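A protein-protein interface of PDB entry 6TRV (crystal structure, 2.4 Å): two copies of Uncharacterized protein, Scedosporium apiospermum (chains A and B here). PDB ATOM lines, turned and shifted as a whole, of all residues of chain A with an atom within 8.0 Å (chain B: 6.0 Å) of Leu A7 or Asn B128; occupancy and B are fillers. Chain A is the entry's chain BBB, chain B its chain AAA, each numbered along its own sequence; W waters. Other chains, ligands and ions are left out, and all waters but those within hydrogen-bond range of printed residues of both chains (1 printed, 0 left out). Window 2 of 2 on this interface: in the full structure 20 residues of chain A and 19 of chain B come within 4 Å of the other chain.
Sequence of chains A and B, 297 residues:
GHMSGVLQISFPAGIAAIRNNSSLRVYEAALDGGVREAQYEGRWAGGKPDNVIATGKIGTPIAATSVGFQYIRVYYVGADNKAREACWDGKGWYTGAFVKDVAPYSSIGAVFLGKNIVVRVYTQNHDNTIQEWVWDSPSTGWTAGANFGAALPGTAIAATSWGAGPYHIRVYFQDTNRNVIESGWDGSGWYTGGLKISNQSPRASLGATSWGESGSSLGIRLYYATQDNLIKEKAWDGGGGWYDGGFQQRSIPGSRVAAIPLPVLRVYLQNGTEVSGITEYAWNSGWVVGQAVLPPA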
ATOM      1  N   SER A   4      34.769   7.585  16.312  1.00  0.00           N
ATOM      2  CA  SER A   4      34.817   6.208  15.625  1.00  0.00           C
ATOM      3  C   SER A   4      34.032   5.200  16.472  1.00  0.00           C
ATOM      4  O   SER A   4      32.904   4.822  16.098  1.00  0.00           O
ATOM      5  CB  SER A   4      36.263   5.694  15.407  1.00  0.00           C
ATOM      6  OG  SER A   4      36.839   6.153  14.183  1.00  0.00           O
ATOM      7  N   GLY A   5      34.634   4.801  17.604  1.00  0.00           N
ATOM      8  CA  GLY A   5      33.990   3.914  18.577  1.00  0.00           C
ATOM      9  C   GLY A   5      32.837   4.595  19.294  1.00  0.00           C
ATOM     10  O   GLY A   5      31.930   3.848  19.728  1.00  0.00           O
ATOM     11  N   VAL A   6      32.865   5.935  19.389  1.00  0.00           N
ATOM     12  CA  VAL A   6      31.862   6.767  20.092  1.00  0.00           C
ATOM     13  C   VAL A   6      30.593   6.855  19.260  1.00  0.00           C
ATOM     14  O   VAL A   6      29.542   7.114  19.761  1.00  0.00           O
ATOM     15  CB  VAL A   6      32.450   8.148  20.452  1.00  0.00           C
ATOM     16  CG1 VAL A   6      32.748   8.977  19.231  1.00  0.00           C
ATOM     17  CG2 VAL A   6      31.552   8.932  21.394  1.00  0.00           C
ATOM     18  N   LEU A   7      30.703   6.624  17.999  1.00  0.00           N
ATOM     19  CA  LEU A   7      29.530   6.632  17.105  1.00  0.00           C
ATOM     20  C   LEU A   7      28.666   5.392  17.323  1.00  0.00           C
ATOM     21  O   LEU A   7      27.565   5.349  16.760  1.00  0.00           O
ATOM     22  CB  LEU A   7      30.044   6.725  15.667  1.00  0.00           C
ATOM     23  CG  LEU A   7      30.477   8.142  15.258  1.00  0.00           C
ATOM     24  CD1 LEU A   7      30.669   8.219  13.718  1.00  0.00           C
ATOM     25  CD2 LEU A   7      29.454   9.186  15.734  1.00  0.00           C
ATOM     26  N   GLN A   8      29.162   4.419  18.087  1.00  0.00           N
ATOM     27  CA  GLN A   8      28.395   3.211  18.448  1.00  0.00           C
ATOM     28  C   GLN A   8      27.417   3.550  19.583  1.00  0.00           C
ATOM     29  O   GLN A   8      26.551   2.740  19.830  1.00  0.00           O
ATOM     30  CB  GLN A   8      29.333   2.092  18.877  1.00  0.00           C
ATOM     31  CG  GLN A   8      30.275   1.557  17.813  1.00  0.00           C
ATOM     32  CD  GLN A   8      31.364   0.717  18.482  1.00  0.00           C
ATOM     33  OE1 GLN A   8      31.973   1.094  19.509  1.00  0.00           O
ATOM     34  NE2 GLN A   8      31.635  -0.453  17.918  1.00  0.00           N
ATOM     35  N   ILE A   9      27.545   4.692  20.253  1.00  0.00           N
ATOM     36  CA  ILE A   9      26.624   5.125  21.360  1.00  0.00           C
ATOM     37  C   ILE A   9      25.339   5.694  20.775  1.00  0.00           C
ATOM     38  O   ILE A   9      25.422   6.520  19.889  1.00  0.00           O
ATOM     39  CB  ILE A   9      27.306   6.165  22.251  1.00  0.00           C
ATOM     40  CG1 ILE A   9      28.688   5.699  22.752  1.00  0.00           C
ATOM     41  CG2 ILE A   9      26.373   6.607  23.347  1.00  0.00           C
ATOM     42  CD1 ILE A   9      28.699   4.393  23.494  1.00  0.00           C
ATOM     43  N   SER A  10      24.206   5.229  21.286  1.00  0.00           N
ATOM     44  CA  SER A  10      22.833   5.654  20.917  1.00  0.00           C
ATOM     45  C   SER A  10      22.688   7.189  20.946  1.00  0.00           C
ATOM     46  O   SER A  10      23.359   7.909  21.704  1.00  0.00           O
ATOM     47  CB  SER A  10      21.789   5.062  21.855  1.00  0.00           C
ATOM     48  OG  SER A  10      21.399   3.762  21.536  1.00  0.00           O
ATOM     49  N   PHE A  11      21.726   7.660  20.188  1.00  0.00           N
ATOM     50  CA  PHE A  11      21.395   9.099  20.016  1.00  0.00           C
ATOM     51  C   PHE A  11      19.878   9.232  20.106  1.00  0.00           C
ATOM     52  O   PHE A  11      19.236   9.119  19.079  1.00  0.00           O
ATOM     53  CB  PHE A  11      21.889   9.598  18.638  1.00  0.00           C
ATOM     54  CG  PHE A  11      21.903  11.096  18.442  1.00  0.00           C
ATOM     55  CD1 PHE A  11      20.754  11.766  18.023  1.00  0.00           C
ATOM     56  CD2 PHE A  11      23.042  11.836  18.712  1.00  0.00           C
ATOM     57  CE1 PHE A  11      20.746  13.147  17.860  1.00  0.00           C
ATOM     58  CE2 PHE A  11      23.036  13.208  18.548  1.00  0.00           C
ATOM     59  CZ  PHE A  11      21.905  13.850  18.110  1.00  0.00           C
ATOM     60  N   ALA A  30      24.830   1.471  23.805  1.00  0.00           N
ATOM     61  CA  ALA A  30      25.186   1.325  22.381  1.00  0.00           C
ATOM     62  C   ALA A  30      23.907   1.201  21.523  1.00  0.00           C
ATOM     63  O   ALA A  30      22.793   0.867  22.030  1.00  0.00           O
ATOM     64  CB  ALA A  30      26.053   0.130  22.163  1.00  0.00           C
ATOM     65  N   LEU A  31      24.054   1.478  20.234  1.00  0.00           N
ATOM     66  CA  LEU A  31      22.890   1.694  19.377  1.00  0.00           C
ATOM     67  C   LEU A  31      22.335   0.339  18.943  1.00  0.00           C
ATOM     68  O   LEU A  31      21.332   0.334  18.267  1.00  0.00           O
ATOM     69  CB  LEU A  31      23.291   2.609  18.229  1.00  0.00           C
ATOM     70  CG  LEU A  31      24.526   2.175  17.462  1.00  0.00           C
ATOM     71  CD1 LEU A  31      24.320   0.817  16.788  1.00  0.00           C
ATOM     72  CD2 LEU A  31      24.883   3.255  16.455  1.00  0.00           C
ATOM     73  N   ARG A  36      27.079  -0.720  28.077  1.00  0.00           N
ATOM     74  CA  ARG A  36      28.552  -0.529  28.196  1.00  0.00           C
ATOM     75  C   ARG A  36      29.009   0.203  29.480  1.00  0.00           C
ATOM     76  O   ARG A  36      28.418   1.220  29.916  1.00  0.00           O
ATOM     77  CB  ARG A  36      29.096   0.240  26.996  1.00  0.00           C
ATOM     78  CG  ARG A  36      28.832  -0.469  25.690  1.00  0.00           C
ATOM     79  CD  ARG A  36      29.820  -0.082  24.638  1.00  0.00           C
ATOM     80  NE  ARG A  36      29.340  -0.647  23.403  1.00  0.00           N
ATOM     81  CZ  ARG A  36      29.810  -0.318  22.220  1.00  0.00           C
ATOM     82  NH1 ARG A  36      30.840   0.514  22.122  1.00  0.00           N
ATOM     83  NH2 ARG A  36      29.258  -0.859  21.161  1.00  0.00           N
ATOM     84  N   THR A 273      28.753  16.617  21.603  1.00  0.00           N
ATOM     85  CA  THR A 273      30.215  16.477  21.523  1.00  0.00           C
ATOM     86  C   THR A 273      30.547  15.133  20.854  1.00  0.00           C
ATOM     87  O   THR A 273      30.120  14.057  21.353  1.00  0.00           O
ATOM     88  CB  THR A 273      30.864  16.631  22.914  1.00  0.00           C
ATOM     89  OG1 THR A 273      30.524  17.916  23.468  1.00  0.00           O
ATOM     90  CG2 THR A 273      32.379  16.479  22.877  1.00  0.00           C
ATOM     91  N   GLU A 274      31.356  15.207  19.786  1.00  0.00           N
ATOM     92  CA  GLU A 274      31.697  14.066  18.898  1.00  0.00           C
ATOM     93  C   GLU A 274      30.402  13.384  18.437  1.00  0.00           C
ATOM     94  O   GLU A 274      30.368  12.172  18.402  1.00  0.00           O
ATOM     95  CB  GLU A 274      32.615  13.097  19.629  1.00  0.00           C
ATOM     96  CG  GLU A 274      33.827  13.777  20.203  1.00  0.00           C
ATOM     97  CD  GLU A 274      35.142  13.141  19.781  1.00  0.00           C
ATOM     98  OE1 GLU A 274      35.312  12.978  18.577  1.00  0.00           O
ATOM     99  OE2 GLU A 274      35.996  12.793  20.634  1.00  0.00           O
ATOM    100  N   VAL A 275      29.369  14.173  18.175  1.00  0.00           N
ATOM    101  CA  VAL A 275      27.975  13.773  17.859  1.00  0.00           C
ATOM    102  C   VAL A 275      27.292  13.050  19.026  1.00  0.00           C
ATOM    103  O   VAL A 275      26.305  13.594  19.525  1.00  0.00           O
ATOM    104  CB  VAL A 275      27.970  12.900  16.617  1.00  0.00           C
ATOM    105  CG1 VAL A 275      26.543  12.608  16.159  1.00  0.00           C
ATOM    106  CG2 VAL A 275      28.788  13.564  15.520  1.00  0.00           C
ATOM    107  N   SER A 276      27.705  11.830  19.375  1.00  0.00           N
ATOM    108  CA  SER A 276      26.918  10.925  20.248  1.00  0.00           C
ATOM    109  C   SER A 276      27.643  10.681  21.584  1.00  0.00           C
ATOM    110  O   SER A 276      27.140   9.917  22.380  1.00  0.00           O
ATOM    111  CB  SER A 276      26.601   9.636  19.513  1.00  0.00           C
ATOM    112  OG  SER A 276      27.797   9.011  19.035  1.00  0.00           O
ATOM    113  N   GLY A 277      28.780  11.333  21.808  1.00  0.00           N
ATOM    114  CA  GLY A 277      29.527  11.267  23.090  1.00  0.00           C
ATOM    115  C   GLY A 277      28.794  11.892  24.305  1.00  0.00           C
ATOM    116  O   GLY A 277      28.161  12.956  24.176  1.00  0.00           O
ATOM    117  N   PRO A 296      33.636   5.436  24.792  1.00  0.00           N
ATOM    118  CA  PRO A 296      34.879   4.970  24.176  1.00  0.00           C
ATOM    119  C   PRO A 296      35.629   6.008  23.321  1.00  0.00           C
ATOM    120  O   PRO A 296      36.551   5.641  22.637  1.00  0.00           O
ATOM    121  CB  PRO A 296      34.356   3.802  23.323  1.00  0.00           C
ATOM    122  CG  PRO A 296      32.946   4.209  22.920  1.00  0.00           C
ATOM    123  CD  PRO A 296      32.422   5.049  24.068  1.00  0.00           C
ATOM    124  N   ALA A 297      35.224   7.272  23.378  1.00  0.00           N
ATOM    125  CA  ALA A 297      35.890   8.386  22.675  1.00  0.00           C
ATOM    126  C   ALA A 297      37.103   8.795  23.496  1.00  0.00           C
ATOM    127  O   ALA A 297      37.310   8.384  24.649  1.00  0.00           O
ATOM    128  CB  ALA A 297      34.973   9.567  22.510  1.00  0.00           C
ATOM    129  OXT ALA A 297      37.888   9.593  22.913  1.00  0.00           O
ATOM    130  N   ALA B 103      25.256   2.580   7.483  1.00  0.00           N
ATOM    131  CA  ALA B 103      25.631   2.865   8.867  1.00  0.00           C
ATOM    132  C   ALA B 103      24.402   2.569   9.718  1.00  0.00           C
ATOM    133  O   ALA B 103      23.266   2.744   9.262  1.00  0.00           O
ATOM    134  CB  ALA B 103      26.111   4.293   8.969  1.00  0.00           C
ATOM    135  N   TYR B 105      23.132   4.132  12.065  1.00  0.00           N
ATOM    136  CA  TYR B 105      22.405   5.405  12.263  1.00  0.00           C
ATOM    137  C   TYR B 105      22.030   6.074  10.943  1.00  0.00           C
ATOM    138  O   TYR B 105      21.711   7.230  11.061  1.00  0.00           O
ATOM    139  CB  TYR B 105      23.282   6.316  13.126  1.00  0.00           C
ATOM    140  CG  TYR B 105      24.719   6.402  12.684  1.00  0.00           C
ATOM    141  CD1 TYR B 105      25.089   6.922  11.470  1.00  0.00           C
ATOM    142  CD2 TYR B 105      25.747   5.994  13.513  1.00  0.00           C
ATOM    143  CE1 TYR B 105      26.429   6.996  11.104  1.00  0.00           C
ATOM    144  CE2 TYR B 105      27.089   6.047  13.155  1.00  0.00           C
ATOM    145  CZ  TYR B 105      27.434   6.559  11.945  1.00  0.00           C
ATOM    146  OH  TYR B 105      28.740   6.660  11.603  1.00  0.00           O
ATOM    147  N   GLN B 124      23.461   6.651   4.101  1.00  0.00           N
ATOM    148  CA  GLN B 124      24.821   6.922   4.665  1.00  0.00           C
ATOM    149  C   GLN B 124      25.582   5.603   4.920  1.00  0.00           C
ATOM    150  O   GLN B 124      25.108   4.730   5.660  1.00  0.00           O
ATOM    151  CB  GLN B 124      24.642   7.717   5.917  1.00  0.00           C
ATOM    152  CG  GLN B 124      25.945   8.155   6.518  1.00  0.00           C
ATOM    153  CD  GLN B 124      25.772   9.269   7.541  1.00  0.00           C
ATOM    154  OE1 GLN B 124      24.986   9.192   8.509  1.00  0.00           O
ATOM    155  NE2 GLN B 124      26.566  10.300   7.357  1.00  0.00           N
ATOM    156  N   ASN B 125      26.683   5.427   4.210  1.00  0.00           N
ATOM    157  CA  ASN B 125      27.685   4.357   4.352  1.00  0.00           C
ATOM    158  C   ASN B 125      28.269   4.312   5.772  1.00  0.00           C
ATOM    159  O   ASN B 125      28.268   5.327   6.461  1.00  0.00           O
ATOM    160  CB  ASN B 125      28.804   4.657   3.341  1.00  0.00           C
ATOM    161  CG  ASN B 125      28.453   4.315   1.894  1.00  0.00           C
ATOM    162  OD1 ASN B 125      27.370   3.749   1.574  1.00  0.00           O
ATOM    163  ND2 ASN B 125      29.414   4.621   1.023  1.00  0.00           N
ATOM    164  N   HIS B 126      28.935   3.228   6.110  1.00  0.00           N
ATOM    165  CA  HIS B 126      29.777   3.094   7.328  1.00  0.00           C
ATOM    166  C   HIS B 126      30.804   4.224   7.376  1.00  0.00           C
ATOM    167  O   HIS B 126      31.102   4.655   8.451  1.00  0.00           O
ATOM    168  CB  HIS B 126      30.395   1.673   7.448  1.00  0.00           C
ATOM    169  CG  HIS B 126      29.340   0.680   7.760  1.00  0.00           C
ATOM    170  ND1 HIS B 126      28.967   0.399   9.056  1.00  0.00           N
ATOM    171  CD2 HIS B 126      28.429   0.078   6.961  1.00  0.00           C
ATOM    172  CE1 HIS B 126      27.930  -0.428   9.030  1.00  0.00           C
ATOM    173  NE2 HIS B 126      27.595  -0.656   7.753  1.00  0.00           N
ATOM    174  N   ASP B 127      31.348   4.667   6.254  1.00  0.00           N
ATOM    175  CA  ASP B 127      32.404   5.701   6.233  1.00  0.00           C
ATOM    176  C   ASP B 127      31.798   7.102   6.375  1.00  0.00           C
ATOM    177  O   ASP B 127      32.596   8.062   6.316  1.00  0.00           O
ATOM    178  CB  ASP B 127      33.250   5.650   4.954  1.00  0.00           C
ATOM    179  CG  ASP B 127      32.577   6.046   3.659  1.00  0.00           C
ATOM    180  OD1 ASP B 127      31.350   6.171   3.609  1.00  0.00           O
ATOM    181  OD2 ASP B 127      33.292   6.137   2.684  1.00  0.00           O
ATOM    182  N   ASN B 128      30.452   7.179   6.426  1.00  0.00           N
ATOM    183  CA  ASN B 128      29.589   8.379   6.684  1.00  0.00           C
ATOM    184  C   ASN B 128      29.453   9.238   5.410  1.00  0.00           C
ATOM    185  O   ASN B 128      28.952  10.326   5.503  1.00  0.00           O
ATOM    186  CB  ASN B 128      30.042   9.207   7.906  1.00  0.00           C
ATOM    187  CG  ASN B 128      30.053   8.461   9.225  1.00  0.00           C
ATOM    188  OD1 ASN B 128      29.125   7.762   9.552  1.00  0.00           O
ATOM    189  ND2 ASN B 128      31.097   8.616  10.001  1.00  0.00           N
ATOM    190  N   THR B 129      29.749   8.713   4.238  1.00  0.00           N
ATOM    191  CA  THR B 129      29.458   9.386   2.946  1.00  0.00           C
ATOM    192  C   THR B 129      28.009   9.142   2.550  1.00  0.00           C
ATOM    193  O   THR B 129      27.436   8.131   2.953  1.00  0.00           O
ATOM    194  CB  THR B 129      30.433   8.974   1.827  1.00  0.00           C
ATOM    195  OG1 THR B 129      30.378   7.578   1.633  1.00  0.00           O
ATOM    196  CG2 THR B 129      31.863   9.327   2.141  1.00  0.00           C
ATOM    197  N   ILE B 130      27.422  10.063   1.772  1.00  0.00           N
ATOM    198  CA  ILE B 130      26.036   9.902   1.226  1.00  0.00           C
ATOM    199  C   ILE B 130      26.208   9.269  -0.137  1.00  0.00           C
ATOM    200  O   ILE B 130      26.852   9.874  -0.957  1.00  0.00           O
ATOM    201  CB  ILE B 130      25.250  11.219   1.137  1.00  0.00           C
ATOM    202  CG1 ILE B 130      25.251  11.919   2.495  1.00  0.00           C
ATOM    203  CG2 ILE B 130      23.826  11.050   0.591  1.00  0.00           C
ATOM    204  CD1 ILE B 130      24.754  11.082   3.610  1.00  0.00           C
ATOM    205  N   GLY B 149      30.181  12.433  -0.807  1.00  0.00           N
ATOM    206  CA  GLY B 149      31.241  12.713   0.184  1.00  0.00           C
ATOM    207  C   GLY B 149      30.761  12.807   1.637  1.00  0.00           C
ATOM    208  O   GLY B 149      29.549  12.502   1.968  1.00  0.00           O
ATOM    209  N   ALA B 150      31.679  13.268   2.502  1.00  0.00           N
ATOM    210  CA  ALA B 150      31.590  13.212   3.980  1.00  0.00           C
ATOM    211  C   ALA B 150      30.367  14.003   4.431  1.00  0.00           C
ATOM    212  O   ALA B 150      30.138  15.090   3.841  1.00  0.00           O
ATOM    213  CB  ALA B 150      32.866  13.733   4.589  1.00  0.00           C
ATOM    214  N   ALA B 151      29.568  13.449   5.347  1.00  0.00           N
ATOM    215  CA  ALA B 151      28.345  14.077   5.911  1.00  0.00           C
ATOM    216  C   ALA B 151      28.349  13.756   7.393  1.00  0.00           C
ATOM    217  O   ALA B 151      29.100  12.822   7.783  1.00  0.00           O
ATOM    218  CB  ALA B 151      27.103  13.583   5.220  1.00  0.00           C
ATOM    219  N   LEU B 152      27.636  14.558   8.181  1.00  0.00           N
ATOM    220  CA  LEU B 152      27.565  14.342   9.626  1.00  0.00           C
ATOM    221  C   LEU B 152      27.083  12.923   9.839  1.00  0.00           C
ATOM    222  O   LEU B 152      26.111  12.524   9.215  1.00  0.00           O
ATOM    223  CB  LEU B 152      26.562  15.287  10.237  1.00  0.00           C
ATOM    224  CG  LEU B 152      26.628  15.353  11.761  1.00  0.00           C
ATOM    225  CD1 LEU B 152      27.301  16.621  12.238  1.00  0.00           C
ATOM    226  CD2 LEU B 152      25.247  15.253  12.363  1.00  0.00           C
ATOM    227  N   PRO B 153      27.720  12.153  10.749  1.00  0.00           N
ATOM    228  CA  PRO B 153      27.221  10.831  11.113  1.00  0.00           C
ATOM    229  C   PRO B 153      25.813  10.917  11.695  1.00  0.00           C
ATOM    230  O   PRO B 153      25.646  11.579  12.683  1.00  0.00           O
ATOM    231  CB  PRO B 153      28.198  10.314  12.177  1.00  0.00           C
ATOM    232  CG  PRO B 153      29.431  11.166  11.964  1.00  0.00           C
ATOM    233  CD  PRO B 153      28.988  12.505  11.406  1.00  0.00           C
ATOM    234  N   GLY B 154      24.861  10.243  11.073  1.00  0.00           N
ATOM    235  CA  GLY B 154      23.475  10.193  11.549  1.00  0.00           C
ATOM    236  C   GLY B 154      22.612  11.231  10.863  1.00  0.00           C
ATOM    237  O   GLY B 154      21.438  11.357  11.281  1.00  0.00           O
ATOM    238  N   ARG B 203      22.198  15.990  13.601  1.00  0.00           N
ATOM    239  CA  ARG B 203      21.158  15.066  13.135  1.00  0.00           C
ATOM    240  C   ARG B 203      19.800  15.735  13.198  1.00  0.00           C
ATOM    241  O   ARG B 203      18.840  15.014  13.245  1.00  0.00           O
ATOM    242  CB  ARG B 203      21.141  13.794  13.976  1.00  0.00           C
ATOM    243  CG  ARG B 203      22.506  13.155  14.130  1.00  0.00           C
ATOM    244  CD  ARG B 203      22.308  11.773  14.631  1.00  0.00           C
ATOM    245  NE  ARG B 203      23.581  11.126  14.811  1.00  0.00           N
ATOM    246  CZ  ARG B 203      23.716   9.884  15.319  1.00  0.00           C
ATOM    247  NH1 ARG B 203      22.653   9.191  15.712  1.00  0.00           N
ATOM    248  NH2 ARG B 203      24.918   9.347  15.495  1.00  0.00           N
HETATM  249  O   HOH W   1      25.298   6.921  17.226  1.00  0.00           O
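Leu A7 touches three residues of chain B. Asn B128 touches just one residue of chain A: Leu A7. Of the printed residues of chain A, Arg B203 touches Phe A11 (3.1 Å) and Val A275 (3.6 Å). Printed residues of chain B within 4 Å of Val A275: Pro B153 and Arg B203. Of the printed residues of chain A, Tyr B105 touches Leu A7. The nearest residue of chain B that does not touch Leu A7 is Arg B203 (4.5 Å). The nearest residue of chain A that does not touch Asn B128 is Ser A4 (7.2 Å). The nearest printed residue of chain A that does not touch Tyr B105 is Leu A31 (4.1 Å).
Water W1 lies within hydrogen-bond range of O of Ile A9 (2.7 Å), O of Leu A7 (2.8 Å) and NH2 of Arg B203 (3.0 Å).
No position is printed for both chains. Of the 6 pairs that touch across the chains among the printed residues, none has its exchanged pair printed and touching as well.
The side-chain hydroxyl of Tyr B105 sits close to the side-chain amide nitrogen of Asn B128, at 3.5 Å. The backbone carbonyl oxygen (O) of Asn B128 lies within hydrogen-bond range of the side-chain amide nitrogen (NE2) of Gln B124, 3.0 Å away. The backbone carbonyl oxygen (O) of Asn B128 sits at hydrogen-bond distance from the backbone NH (N) of Ala B151, 3.2 Å away. The backbone carbonyl oxygen of Pro B153 sits at hydrogen-bond distance from the guanidinium group of Arg B203, 3.0 Å away.
Among the printed residues, merely in contact across the chains: Leu A7 with Tyr B105 (3.3 Å), Leu A7 with Asn B128 (3.8 Å), Leu A7 with Pro B153 (3.6 Å), Phe A11 with Arg B203 (3.1 Å), Val A275 with Pro B153 (3.7 Å) and Val A275 with Arg B203 (3.6 Å).
Of the 18 printed residues of chain A, 3 touch a printed residue of chain B. Printed residues of chain A that touch a printed residue of chain B: Leu A7, Phe A11 and Val A275. Hydrophobic or aromatic side chains of chain A within 4 Å of the printed part of chain B: Leu A7, Phe A11 and Val A275. Of the 16 printed residues of chain B, 4 touch a printed residue of chain A. Printed residues of chain B that touch a printed residue of chain A: Tyr B105, Asn B128, Pro B153 and Arg B203. Hydrophobic or aromatic side chains of chain B within 4 Å of the printed part of chain A: Tyr B105 and Pro B153. Among the printed residues, 6 pairs touch across the chains. Among the printed residues, no Asp or Glu carboxylate lies within 4 Å of a Lys or Arg side-chain nitrogen of the other chain.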
